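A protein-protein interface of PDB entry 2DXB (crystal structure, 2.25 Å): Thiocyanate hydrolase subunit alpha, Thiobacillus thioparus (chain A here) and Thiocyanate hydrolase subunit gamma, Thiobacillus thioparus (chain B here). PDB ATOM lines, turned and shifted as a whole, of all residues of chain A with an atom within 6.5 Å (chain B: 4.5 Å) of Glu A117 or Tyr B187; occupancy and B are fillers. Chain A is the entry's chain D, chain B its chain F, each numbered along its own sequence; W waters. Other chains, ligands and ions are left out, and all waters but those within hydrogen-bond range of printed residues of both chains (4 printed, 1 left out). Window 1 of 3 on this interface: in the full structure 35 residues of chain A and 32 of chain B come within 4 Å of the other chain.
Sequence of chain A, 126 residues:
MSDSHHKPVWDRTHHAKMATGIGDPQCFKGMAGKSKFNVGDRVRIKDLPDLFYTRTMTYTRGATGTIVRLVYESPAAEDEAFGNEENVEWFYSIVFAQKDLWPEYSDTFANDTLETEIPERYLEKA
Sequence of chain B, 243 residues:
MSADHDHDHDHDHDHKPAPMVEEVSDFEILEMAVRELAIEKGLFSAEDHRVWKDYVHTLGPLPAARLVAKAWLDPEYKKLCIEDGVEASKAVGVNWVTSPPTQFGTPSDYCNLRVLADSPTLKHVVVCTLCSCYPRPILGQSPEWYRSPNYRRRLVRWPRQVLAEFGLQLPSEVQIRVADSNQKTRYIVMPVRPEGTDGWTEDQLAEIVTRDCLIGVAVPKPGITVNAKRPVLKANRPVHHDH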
ATOM      1  N   ARG A  55      17.274  21.485  19.095  1.00  0.00           N
ATOM      2  CA  ARG A  55      18.389  21.811  18.214  1.00  0.00           C
ATOM      3  C   ARG A  55      17.924  22.824  17.171  1.00  0.00           C
ATOM      4  O   ARG A  55      18.533  22.981  16.110  1.00  0.00           O
ATOM      5  CB  ARG A  55      18.969  20.557  17.556  1.00  0.00           C
ATOM      6  CG  ARG A  55      19.651  19.622  18.565  1.00  0.00           C
ATOM      7  CD  ARG A  55      20.494  18.557  17.886  1.00  0.00           C
ATOM      8  NE  ARG A  55      21.753  19.072  17.354  1.00  0.00           N
ATOM      9  CZ  ARG A  55      22.782  19.466  18.100  1.00  0.00           C
ATOM     10  NH1 ARG A  55      22.715  19.415  19.429  1.00  0.00           N
ATOM     11  NH2 ARG A  55      23.887  19.905  17.515  1.00  0.00           N
ATOM     12  N   THR A  56      16.830  23.507  17.492  1.00  0.00           N
ATOM     13  CA  THR A  56      16.290  24.544  16.623  1.00  0.00           C
ATOM     14  C   THR A  56      16.589  25.846  17.362  1.00  0.00           C
ATOM     15  O   THR A  56      15.871  26.229  18.290  1.00  0.00           O
ATOM     16  CB  THR A  56      14.768  24.370  16.420  1.00  0.00           C
ATOM     17  OG1 THR A  56      14.525  23.134  15.729  1.00  0.00           O
ATOM     18  CG2 THR A  56      14.191  25.526  15.597  1.00  0.00           C
ATOM     19  N   MET A  57      17.674  26.499  16.958  1.00  0.00           N
ATOM     20  CA  MET A  57      18.130  27.733  17.595  1.00  0.00           C
ATOM     21  C   MET A  57      17.064  28.791  17.865  1.00  0.00           C
ATOM     22  O   MET A  57      16.175  29.045  17.044  1.00  0.00           O
ATOM     23  CB  MET A  57      19.256  28.362  16.774  1.00  0.00           C
ATOM     24  CG  MET A  57      20.504  27.501  16.642  1.00  0.00           C
ATOM     25  SD  MET A  57      20.284  26.056  15.588  1.00  0.00           S
ATOM     26  CE  MET A  57      20.049  26.820  13.968  1.00  0.00           C
ATOM     27  N   VAL A  71      16.961  17.321   3.082  1.00  0.00           N
ATOM     28  CA  VAL A  71      18.228  16.635   3.295  1.00  0.00           C
ATOM     29  C   VAL A  71      18.205  15.153   3.636  1.00  0.00           C
ATOM     30  O   VAL A  71      19.042  14.397   3.132  1.00  0.00           O
ATOM     31  CB  VAL A  71      19.078  17.392   4.339  1.00  0.00           C
ATOM     32  CG1 VAL A  71      19.443  18.770   3.787  1.00  0.00           C
ATOM     33  CG2 VAL A  71      18.315  17.534   5.645  1.00  0.00           C
ATOM     34  N   TYR A  72      17.269  14.730   4.476  1.00  0.00           N
ATOM     35  CA  TYR A  72      17.179  13.321   4.850  1.00  0.00           C
ATOM     36  C   TYR A  72      16.054  13.094   5.846  1.00  0.00           C
ATOM     37  O   TYR A  72      15.335  14.023   6.218  1.00  0.00           O
ATOM     38  CB  TYR A  72      18.504  12.847   5.464  1.00  0.00           C
ATOM     39  CG  TYR A  72      18.991  13.733   6.589  1.00  0.00           C
ATOM     40  CD1 TYR A  72      18.315  13.776   7.810  1.00  0.00           C
ATOM     41  CD2 TYR A  72      20.087  14.582   6.410  1.00  0.00           C
ATOM     42  CE1 TYR A  72      18.707  14.650   8.823  1.00  0.00           C
ATOM     43  CE2 TYR A  72      20.490  15.458   7.414  1.00  0.00           C
ATOM     44  CZ  TYR A  72      19.792  15.489   8.614  1.00  0.00           C
ATOM     45  OH  TYR A  72      20.153  16.377   9.596  1.00  0.00           O
ATOM     46  N   PHE A  91      13.752  16.230   7.406  1.00  0.00           N
ATOM     47  CA  PHE A  91      14.567  17.360   7.830  1.00  0.00           C
ATOM     48  C   PHE A  91      14.746  18.244   6.609  1.00  0.00           C
ATOM     49  O   PHE A  91      14.935  17.751   5.498  1.00  0.00           O
ATOM     50  CB  PHE A  91      15.935  16.900   8.336  1.00  0.00           C
ATOM     51  CG  PHE A  91      15.940  16.489   9.780  1.00  0.00           C
ATOM     52  CD1 PHE A  91      15.215  15.381  10.206  1.00  0.00           C
ATOM     53  CD2 PHE A  91      16.684  17.203  10.714  1.00  0.00           C
ATOM     54  CE1 PHE A  91      15.233  14.986  11.551  1.00  0.00           C
ATOM     55  CE2 PHE A  91      16.711  16.820  12.060  1.00  0.00           C
ATOM     56  CZ  PHE A  91      15.985  15.709  12.479  1.00  0.00           C
ATOM     57  N   TYR A  92      14.688  19.550   6.823  1.00  0.00           N
ATOM     58  CA  TYR A  92      14.806  20.502   5.734  1.00  0.00           C
ATOM     59  C   TYR A  92      15.938  21.499   5.923  1.00  0.00           C
ATOM     60  O   TYR A  92      16.200  21.959   7.038  1.00  0.00           O
ATOM     61  CB  TYR A  92      13.500  21.282   5.603  1.00  0.00           C
ATOM     62  CG  TYR A  92      12.269  20.426   5.411  1.00  0.00           C
ATOM     63  CD1 TYR A  92      11.782  20.147   4.135  1.00  0.00           C
ATOM     64  CD2 TYR A  92      11.575  19.915   6.510  1.00  0.00           C
ATOM     65  CE1 TYR A  92      10.629  19.387   3.954  1.00  0.00           C
ATOM     66  CE2 TYR A  92      10.424  19.149   6.341  1.00  0.00           C
ATOM     67  CZ  TYR A  92       9.955  18.894   5.060  1.00  0.00           C
ATOM     68  OH  TYR A  92       8.799  18.167   4.889  1.00  0.00           O
ATOM     69  N   SER A  93      16.612  21.832   4.832  1.00  0.00           N
ATOM     70  CA  SER A  93      17.660  22.831   4.896  1.00  0.00           C
ATOM     71  C   SER A  93      16.932  24.118   4.504  1.00  0.00           C
ATOM     72  O   SER A  93      16.331  24.200   3.425  1.00  0.00           O
ATOM     73  CB  SER A  93      18.775  22.522   3.906  1.00  0.00           C
ATOM     74  OG  SER A  93      19.893  23.353   4.165  1.00  0.00           O
ATOM     75  N   ILE A  94      16.969  25.108   5.389  1.00  0.00           N
ATOM     76  CA  ILE A  94      16.277  26.369   5.166  1.00  0.00           C
ATOM     77  C   ILE A  94      17.215  27.572   5.109  1.00  0.00           C
ATOM     78  O   ILE A  94      18.174  27.669   5.881  1.00  0.00           O
ATOM     79  CB  ILE A  94      15.235  26.589   6.281  1.00  0.00           C
ATOM     80  CG1 ILE A  94      14.221  25.440   6.259  1.00  0.00           C
ATOM     81  CG2 ILE A  94      14.550  27.935   6.110  1.00  0.00           C
ATOM     82  CD1 ILE A  94      13.360  25.364   7.486  1.00  0.00           C
ATOM     83  N   GLU A 115      21.987  29.529   6.331  1.00  0.00           N
ATOM     84  CA  GLU A 115      21.365  28.238   6.039  1.00  0.00           C
ATOM     85  C   GLU A 115      21.539  27.261   7.197  1.00  0.00           C
ATOM     86  O   GLU A 115      22.646  27.074   7.706  1.00  0.00           O
ATOM     87  CB  GLU A 115      21.973  27.628   4.769  1.00  0.00           C
ATOM     88  CG  GLU A 115      21.292  26.341   4.310  1.00  0.00           C
ATOM     89  CD  GLU A 115      21.795  25.847   2.963  1.00  0.00           C
ATOM     90  OE1 GLU A 115      22.548  26.582   2.286  1.00  0.00           O
ATOM     91  OE2 GLU A 115      21.427  24.719   2.574  1.00  0.00           O
ATOM     92  N   THR A 116      20.444  26.636   7.609  1.00  0.00           N
ATOM     93  CA  THR A 116      20.496  25.676   8.702  1.00  0.00           C
ATOM     94  C   THR A 116      19.394  24.626   8.517  1.00  0.00           C
ATOM     95  O   THR A 116      18.474  24.815   7.712  1.00  0.00           O
ATOM     96  CB  THR A 116      20.356  26.399  10.067  1.00  0.00           C
ATOM     97  OG1 THR A 116      20.603  25.474  11.132  1.00  0.00           O
ATOM     98  CG2 THR A 116      18.966  26.997  10.220  1.00  0.00           C
ATOM     99  N   GLU A 117      19.487  23.517   9.246  1.00  0.00           N
ATOM    100  CA  GLU A 117      18.496  22.459   9.104  1.00  0.00           C
ATOM    101  C   GLU A 117      17.482  22.428  10.234  1.00  0.00           C
ATOM    102  O   GLU A 117      17.824  22.611  11.404  1.00  0.00           O
ATOM    103  CB  GLU A 117      19.195  21.103   8.973  1.00  0.00           C
ATOM    104  CG  GLU A 117      20.231  21.080   7.843  1.00  0.00           C
ATOM    105  CD  GLU A 117      20.806  19.699   7.567  1.00  0.00           C
ATOM    106  OE1 GLU A 117      20.854  18.864   8.499  1.00  0.00           O
ATOM    107  OE2 GLU A 117      21.230  19.458   6.414  1.00  0.00           O
ATOM    108  N   ILE A 118      16.223  22.198   9.866  1.00  0.00           N
ATOM    109  CA  ILE A 118      15.133  22.152  10.823  1.00  0.00           C
ATOM    110  C   ILE A 118      14.220  20.964  10.538  1.00  0.00           C
ATOM    111  O   ILE A 118      13.852  20.718   9.389  1.00  0.00           O
ATOM    112  CB  ILE A 118      14.255  23.426  10.738  1.00  0.00           C
ATOM    113  CG1 ILE A 118      15.121  24.693  10.766  1.00  0.00           C
ATOM    114  CG2 ILE A 118      13.245  23.427  11.874  1.00  0.00           C
ATOM    115  CD1 ILE A 118      15.770  24.984  12.089  1.00  0.00           C
ATOM    116  N   PRO A 119      13.844  20.205  11.582  1.00  0.00           N
ATOM    117  CA  PRO A 119      12.958  19.059  11.359  1.00  0.00           C
ATOM    118  C   PRO A 119      11.536  19.570  11.085  1.00  0.00           C
ATOM    119  O   PRO A 119      11.130  20.615  11.593  1.00  0.00           O
ATOM    120  CB  PRO A 119      13.072  18.275  12.665  1.00  0.00           C
ATOM    121  CG  PRO A 119      13.313  19.355  13.682  1.00  0.00           C
ATOM    122  CD  PRO A 119      14.310  20.251  12.980  1.00  0.00           C
ATOM    123  N   LEU B 113      27.561  14.395   4.422  1.00  0.00           N
ATOM    124  CA  LEU B 113      28.436  15.510   4.103  1.00  0.00           C
ATOM    125  C   LEU B 113      27.855  16.294   2.940  1.00  0.00           C
ATOM    126  O   LEU B 113      27.405  15.710   1.958  1.00  0.00           O
ATOM    127  CB  LEU B 113      29.824  15.014   3.686  1.00  0.00           C
ATOM    128  CG  LEU B 113      30.715  16.089   3.048  1.00  0.00           C
ATOM    129  CD1 LEU B 113      31.210  17.041   4.133  1.00  0.00           C
ATOM    130  CD2 LEU B 113      31.901  15.443   2.337  1.00  0.00           C
ATOM    131  N   ARG B 114      27.852  17.616   3.058  1.00  0.00           N
ATOM    132  CA  ARG B 114      27.392  18.461   1.969  1.00  0.00           C
ATOM    133  C   ARG B 114      28.535  19.404   1.633  1.00  0.00           C
ATOM    134  O   ARG B 114      29.222  19.910   2.525  1.00  0.00           O
ATOM    135  CB  ARG B 114      26.145  19.267   2.352  1.00  0.00           C
ATOM    136  CG  ARG B 114      24.831  18.489   2.238  1.00  0.00           C
ATOM    137  CD  ARG B 114      23.641  19.438   2.231  1.00  0.00           C
ATOM    138  NE  ARG B 114      23.681  20.338   1.079  1.00  0.00           N
ATOM    139  CZ  ARG B 114      23.200  21.579   1.078  1.00  0.00           C
ATOM    140  NH1 ARG B 114      22.634  22.081   2.170  1.00  0.00           N
ATOM    141  NH2 ARG B 114      23.299  22.328  -0.012  1.00  0.00           N
ATOM    142  N   LEU B 116      29.576  22.920   0.013  1.00  0.00           N
ATOM    143  CA  LEU B 116      29.041  24.231  -0.323  1.00  0.00           C
ATOM    144  C   LEU B 116      29.979  24.903  -1.322  1.00  0.00           C
ATOM    145  O   LEU B 116      31.112  25.265  -0.990  1.00  0.00           O
ATOM    146  CB  LEU B 116      28.908  25.074   0.950  1.00  0.00           C
ATOM    147  CG  LEU B 116      28.083  24.426   2.073  1.00  0.00           C
ATOM    148  CD1 LEU B 116      28.086  25.317   3.308  1.00  0.00           C
ATOM    149  CD2 LEU B 116      26.649  24.181   1.591  1.00  0.00           C
ATOM    150  N   VAL B 126      31.313  28.263   7.610  1.00  0.00           N
ATOM    151  CA  VAL B 126      30.641  27.290   8.465  1.00  0.00           C
ATOM    152  C   VAL B 126      30.869  27.437   9.967  1.00  0.00           C
ATOM    153  O   VAL B 126      31.919  27.901  10.412  1.00  0.00           O
ATOM    154  CB  VAL B 126      31.049  25.852   8.050  1.00  0.00           C
ATOM    155  CG1 VAL B 126      30.213  24.819   8.805  1.00  0.00           C
ATOM    156  CG2 VAL B 126      30.882  25.686   6.545  1.00  0.00           C
ATOM    157  N   PRO B 135      33.179  18.240   9.977  1.00  0.00           N
ATOM    158  CA  PRO B 135      33.299  17.064   9.101  1.00  0.00           C
ATOM    159  C   PRO B 135      34.605  16.282   9.318  1.00  0.00           C
ATOM    160  O   PRO B 135      35.407  16.120   8.392  1.00  0.00           O
ATOM    161  CB  PRO B 135      33.219  17.680   7.709  1.00  0.00           C
ATOM    162  CG  PRO B 135      33.944  18.969   7.890  1.00  0.00           C
ATOM    163  CD  PRO B 135      33.365  19.485   9.204  1.00  0.00           C
ATOM    164  N   ALA B 179      26.613  28.856   7.193  1.00  0.00           N
ATOM    165  CA  ALA B 179      25.947  27.567   7.328  1.00  0.00           C
ATOM    166  C   ALA B 179      26.128  27.109   8.772  1.00  0.00           C
ATOM    167  O   ALA B 179      27.253  26.937   9.235  1.00  0.00           O
ATOM    168  CB  ALA B 179      26.551  26.553   6.374  1.00  0.00           C
ATOM    169  N   ASP B 180      25.015  26.935   9.479  1.00  0.00           N
ATOM    170  CA  ASP B 180      25.044  26.489  10.867  1.00  0.00           C
ATOM    171  C   ASP B 180      24.688  25.002  10.873  1.00  0.00           C
ATOM    172  O   ASP B 180      23.537  24.643  10.637  1.00  0.00           O
ATOM    173  CB  ASP B 180      24.015  27.288  11.680  1.00  0.00           C
ATOM    174  CG  ASP B 180      24.117  27.041  13.179  1.00  0.00           C
ATOM    175  OD1 ASP B 180      24.824  26.098  13.593  1.00  0.00           O
ATOM    176  OD2 ASP B 180      23.477  27.790  13.945  1.00  0.00           O
ATOM    177  N   SER B 181      25.668  24.133  11.120  1.00  0.00           N
ATOM    178  CA  SER B 181      25.398  22.693  11.136  1.00  0.00           C
ATOM    179  C   SER B 181      24.847  22.240  12.477  1.00  0.00           C
ATOM    180  O   SER B 181      25.576  21.732  13.324  1.00  0.00           O
ATOM    181  CB  SER B 181      26.661  21.895  10.789  1.00  0.00           C
ATOM    182  OG  SER B 181      27.825  22.644  11.054  1.00  0.00           O
ATOM    183  N   ASN B 182      23.541  22.404  12.641  1.00  0.00           N
ATOM    184  CA  ASN B 182      22.863  22.066  13.882  1.00  0.00           C
ATOM    185  C   ASN B 182      22.212  20.684  13.915  1.00  0.00           C
ATOM    186  O   ASN B 182      21.669  20.290  14.942  1.00  0.00           O
ATOM    187  CB  ASN B 182      21.804  23.127  14.167  1.00  0.00           C
ATOM    188  CG  ASN B 182      20.730  23.162  13.100  1.00  0.00           C
ATOM    189  OD1 ASN B 182      21.021  22.991  11.911  1.00  0.00           O
ATOM    190  ND2 ASN B 182      19.484  23.381  13.513  1.00  0.00           N
ATOM    191  N   GLN B 183      22.237  19.953  12.808  1.00  0.00           N
ATOM    192  CA  GLN B 183      21.631  18.623  12.809  1.00  0.00           C
ATOM    193  C   GLN B 183      22.661  17.567  12.386  1.00  0.00           C
ATOM    194  O   GLN B 183      23.804  17.602  12.843  1.00  0.00           O
ATOM    195  CB  GLN B 183      20.393  18.590  11.899  1.00  0.00           C
ATOM    196  CG  GLN B 183      19.318  19.643  12.216  1.00  0.00           C
ATOM    197  CD  GLN B 183      18.647  19.468  13.580  1.00  0.00           C
ATOM    198  OE1 GLN B 183      18.777  18.427  14.231  1.00  0.00           O
ATOM    199  NE2 GLN B 183      17.908  20.488  14.007  1.00  0.00           N
ATOM    200  N   LYS B 184      22.285  16.644  11.504  1.00  0.00           N
ATOM    201  CA  LYS B 184      23.218  15.594  11.098  1.00  0.00           C
ATOM    202  C   LYS B 184      24.105  15.886   9.889  1.00  0.00           C
ATOM    203  O   LYS B 184      24.966  15.079   9.535  1.00  0.00           O
ATOM    204  CB  LYS B 184      22.457  14.281  10.894  1.00  0.00           C
ATOM    205  CG  LYS B 184      21.861  13.743  12.193  1.00  0.00           C
ATOM    206  CD  LYS B 184      21.207  12.384  12.016  1.00  0.00           C
ATOM    207  CE  LYS B 184      20.774  11.813  13.364  1.00  0.00           C
ATOM    208  NZ  LYS B 184      20.194  10.448  13.237  1.00  0.00           N
ATOM    209  N   THR B 185      23.911  17.039   9.266  1.00  0.00           N
ATOM    210  CA  THR B 185      24.721  17.403   8.110  1.00  0.00           C
ATOM    211  C   THR B 185      26.021  18.093   8.531  1.00  0.00           C
ATOM    212  O   THR B 185      26.041  18.873   9.484  1.00  0.00           O
ATOM    213  CB  THR B 185      23.949  18.355   7.169  1.00  0.00           C
ATOM    214  OG1 THR B 185      22.888  17.639   6.523  1.00  0.00           O
ATOM    215  CG2 THR B 185      24.879  18.943   6.114  1.00  0.00           C
ATOM    216  N   ARG B 186      27.103  17.785   7.825  1.00  0.00           N
ATOM    217  CA  ARG B 186      28.405  18.401   8.071  1.00  0.00           C
ATOM    218  C   ARG B 186      28.781  19.043   6.739  1.00  0.00           C
ATOM    219  O   ARG B 186      28.420  18.523   5.682  1.00  0.00           O
ATOM    220  CB  ARG B 186      29.446  17.348   8.479  1.00  0.00           C
ATOM    221  CG  ARG B 186      29.129  16.634   9.791  1.00  0.00           C
ATOM    222  CD  ARG B 186      29.177  17.572  10.987  1.00  0.00           C
ATOM    223  NE  ARG B 186      28.768  16.899  12.221  1.00  0.00           N
ATOM    224  CZ  ARG B 186      27.519  16.833  12.668  1.00  0.00           C
ATOM    225  NH1 ARG B 186      26.530  17.408  11.988  1.00  0.00           N
ATOM    226  NH2 ARG B 186      27.254  16.185  13.796  1.00  0.00           N
ATOM    227  N   TYR B 187      29.494  20.167   6.779  1.00  0.00           N
ATOM    228  CA  TYR B 187      29.859  20.859   5.543  1.00  0.00           C
ATOM    229  C   TYR B 187      31.336  21.177   5.394  1.00  0.00           C
ATOM    230  O   TYR B 187      32.063  21.319   6.380  1.00  0.00           O
ATOM    231  CB  TYR B 187      29.155  22.222   5.435  1.00  0.00           C
ATOM    232  CG  TYR B 187      27.676  22.288   5.730  1.00  0.00           C
ATOM    233  CD1 TYR B 187      26.728  22.081   4.725  1.00  0.00           C
ATOM    234  CD2 TYR B 187      27.222  22.626   7.006  1.00  0.00           C
ATOM    235  CE1 TYR B 187      25.365  22.214   4.984  1.00  0.00           C
ATOM    236  CE2 TYR B 187      25.868  22.761   7.275  1.00  0.00           C
ATOM    237  CZ  TYR B 187      24.943  22.554   6.262  1.00  0.00           C
ATOM    238  OH  TYR B 187      23.605  22.679   6.542  1.00  0.00           O
ATOM    239  N   ILE B 188      31.765  21.289   4.139  1.00  0.00           N
ATOM    240  CA  ILE B 188      33.111  21.733   3.813  1.00  0.00           C
ATOM    241  C   ILE B 188      32.836  22.770   2.734  1.00  0.00           C
ATOM    242  O   ILE B 188      31.857  22.654   1.983  1.00  0.00           O
ATOM    243  CB  ILE B 188      34.059  20.632   3.242  1.00  0.00           C
ATOM    244  CG1 ILE B 188      33.412  19.902   2.072  1.00  0.00           C
ATOM    245  CG2 ILE B 188      34.495  19.689   4.350  1.00  0.00           C
ATOM    246  CD1 ILE B 188      34.370  18.936   1.394  1.00  0.00           C
ATOM    247  N   VAL B 189      33.672  23.796   2.668  1.00  0.00           N
ATOM    248  CA  VAL B 189      33.482  24.844   1.682  1.00  0.00           C
ATOM    249  C   VAL B 189      34.378  24.650   0.468  1.00  0.00           C
ATOM    250  O   VAL B 189      35.573  24.394   0.604  1.00  0.00           O
ATOM    251  CB  VAL B 189      33.773  26.232   2.291  1.00  0.00           C
ATOM    252  CG1 VAL B 189      33.666  27.308   1.210  1.00  0.00           C
ATOM    253  CG2 VAL B 189      32.796  26.515   3.432  1.00  0.00           C
HETATM  254  O   HOH W   1      23.584  19.966  10.177  1.00  0.00           O
HETATM  255  O   HOH W   2      23.047  25.271   0.068  1.00  0.00           O
HETATM  256  O   HOH W   3      15.610  20.665  16.419  1.00  0.00           O
HETATM  257  O   HOH W   4      22.028  21.640   4.791  1.00  0.00           O
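NE of Arg A55 lies within hydrogen-bond range of O of Asn B182 (2.7 Å).
The side-chain amide nitrogen (NE2) of Gln B183 is in hydrogen-bond range of the backbone carbonyl oxygen (O) of Arg A55, 3.3 Å away.
The side-chain amide nitrogen (ND2) of Asn B182 sits at hydrogen-bond distance from the side-chain sulfur (SD) of Met A57.
OH of Tyr A72 sits at hydrogen-bond distance from N of Lys B184 (2.9 Å).
OE2 of Glu A115 is in salt-bridge range of NH1 of Arg B114.
O of Glu A115 lies within hydrogen-bond range of N of Asp B180 (3.0 Å).
The backbone carbonyl oxygen (O) of Asp B180 sits at hydrogen-bond distance from the side-chain hydroxyl (OG1) of Thr A116, at 3.1 Å.
The side-chain hydroxyl (OG1) of Thr A116 lies within hydrogen-bond range of the side-chain amide oxygen (OD1) of Asn B182.
O of Glu A117 is in hydrogen-bond range of ND2 of Asn B182 (2.8 Å).
NE2 of Gln B183 is in hydrogen-bond range of O of Glu A117.
The side-chain carboxylate of Glu A117 is in hydrogen-bond range of the side-chain hydroxyl of Thr B185.
The side-chain hydroxyl of Tyr A72 lies within hydrogen-bond range of the side-chain carboxylate of Glu A117, 2.8 Å away.
The side-chain carboxylate of Glu A115 is in hydrogen-bond range of the side-chain hydroxyl of Ser A93, at 2.6 Å.
The backbone carbonyl oxygen of Thr A116 sits at hydrogen-bond distance from the backbone NH of Ile A94, 2.8 Å away.
O of Arg B186 lies within hydrogen-bond range of N of Arg B114 (2.8 Å).
The backbone carbonyl oxygen of Asp B180 sits close to the side-chain amide oxygen of Asn B182.
The side-chain amide nitrogen of Asn B182 sits close to the side-chain amide nitrogen of Gln B183, 3.3 Å away.
Asp B180 touches Met A57.
CB of Gln B183 touches OH of Tyr A72, at 3.2 Å.
OG1 of Thr B185 touches CE2 of Tyr A72, at 3.4 Å.
OE1 of Gln B183 touches CE2 of Phe A91, at 3.4 Å.
Arg B114 touches Ser A93.
Glu A115 touches Ala B179.
CG of Glu A117 touches OH of Tyr B187 (3.95 Å).
Pro A119 touches Gln B183.
Of the printed residues of chain B, Arg A55 touches Asn B182 and Gln B183.
Of the printed residues of chain B, Glu A117 touches Asn B182 (2.8 Å), Gln B183 (3.4 Å), Thr B185 (2.5 Å) and Tyr B187 (3.95 Å).
Of the printed residues of chain A, Ala B179 touches Glu A115.
Of the printed residues of chain A, Asp B180 touches Met A57 (3.6 Å), Glu A115 (3.0 Å) and Thr A116 (3.1 Å).
Printed residues of chain A within 4 Å of Lys B184: Tyr A72 (2.9 Å).
Tyr B187 touches one residue of chain A.
Ile B188 touches none of the printed residues of chain A.
Val B189 touches none of the printed residues of chain A.
The nearest printed residue of chain B that does not touch Glu A117 is Lys B184 (4.001 Å).
Hydrophobic or aromatic side chains of chain B that line the printed part of chain A: Tyr B187.
Along chain B the printed residues that touch a printed residue of chain A span positions 114 to 187.
Of the 14 printed residues of chain A, 9 touch a printed residue of chain B.
Hydrophobic or aromatic side chains of chain A within 4 Å of the printed part of chain B: Met A57, Tyr A72, Phe A91 and Pro A119.
Among the printed residues, 19 pairs touch across the chains.
Water W4 lies within hydrogen-bond range of the side-chain hydroxyl (OH) of Tyr B187, the guanidinium group (NH1) of Arg B114, the side-chain hydroxyl (OG) of Ser A93 and the side-chain carboxylate (OE2) of Glu A117.
Water W2 lies within hydrogen-bond range of the side-chain carboxylate of Glu A115 (2.6 Å) and the guanidinium group of Arg B114 (3.0 Å).
Water W1 lies within hydrogen-bond range of the backbone carbonyl oxygen (O) of Thr B185, the backbone NH (N) of Gln B183, the side-chain carboxylate (OE1) of Glu A117 and the backbone NH (N) of Asn B182.
Water W3 lies within hydrogen-bond range of the side-chain hydroxyl of Thr A56 (2.8 Å), the backbone NH of Arg A55 (3.3 Å) and the side-chain amide nitrogen of Gln B183 (3.3 Å).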
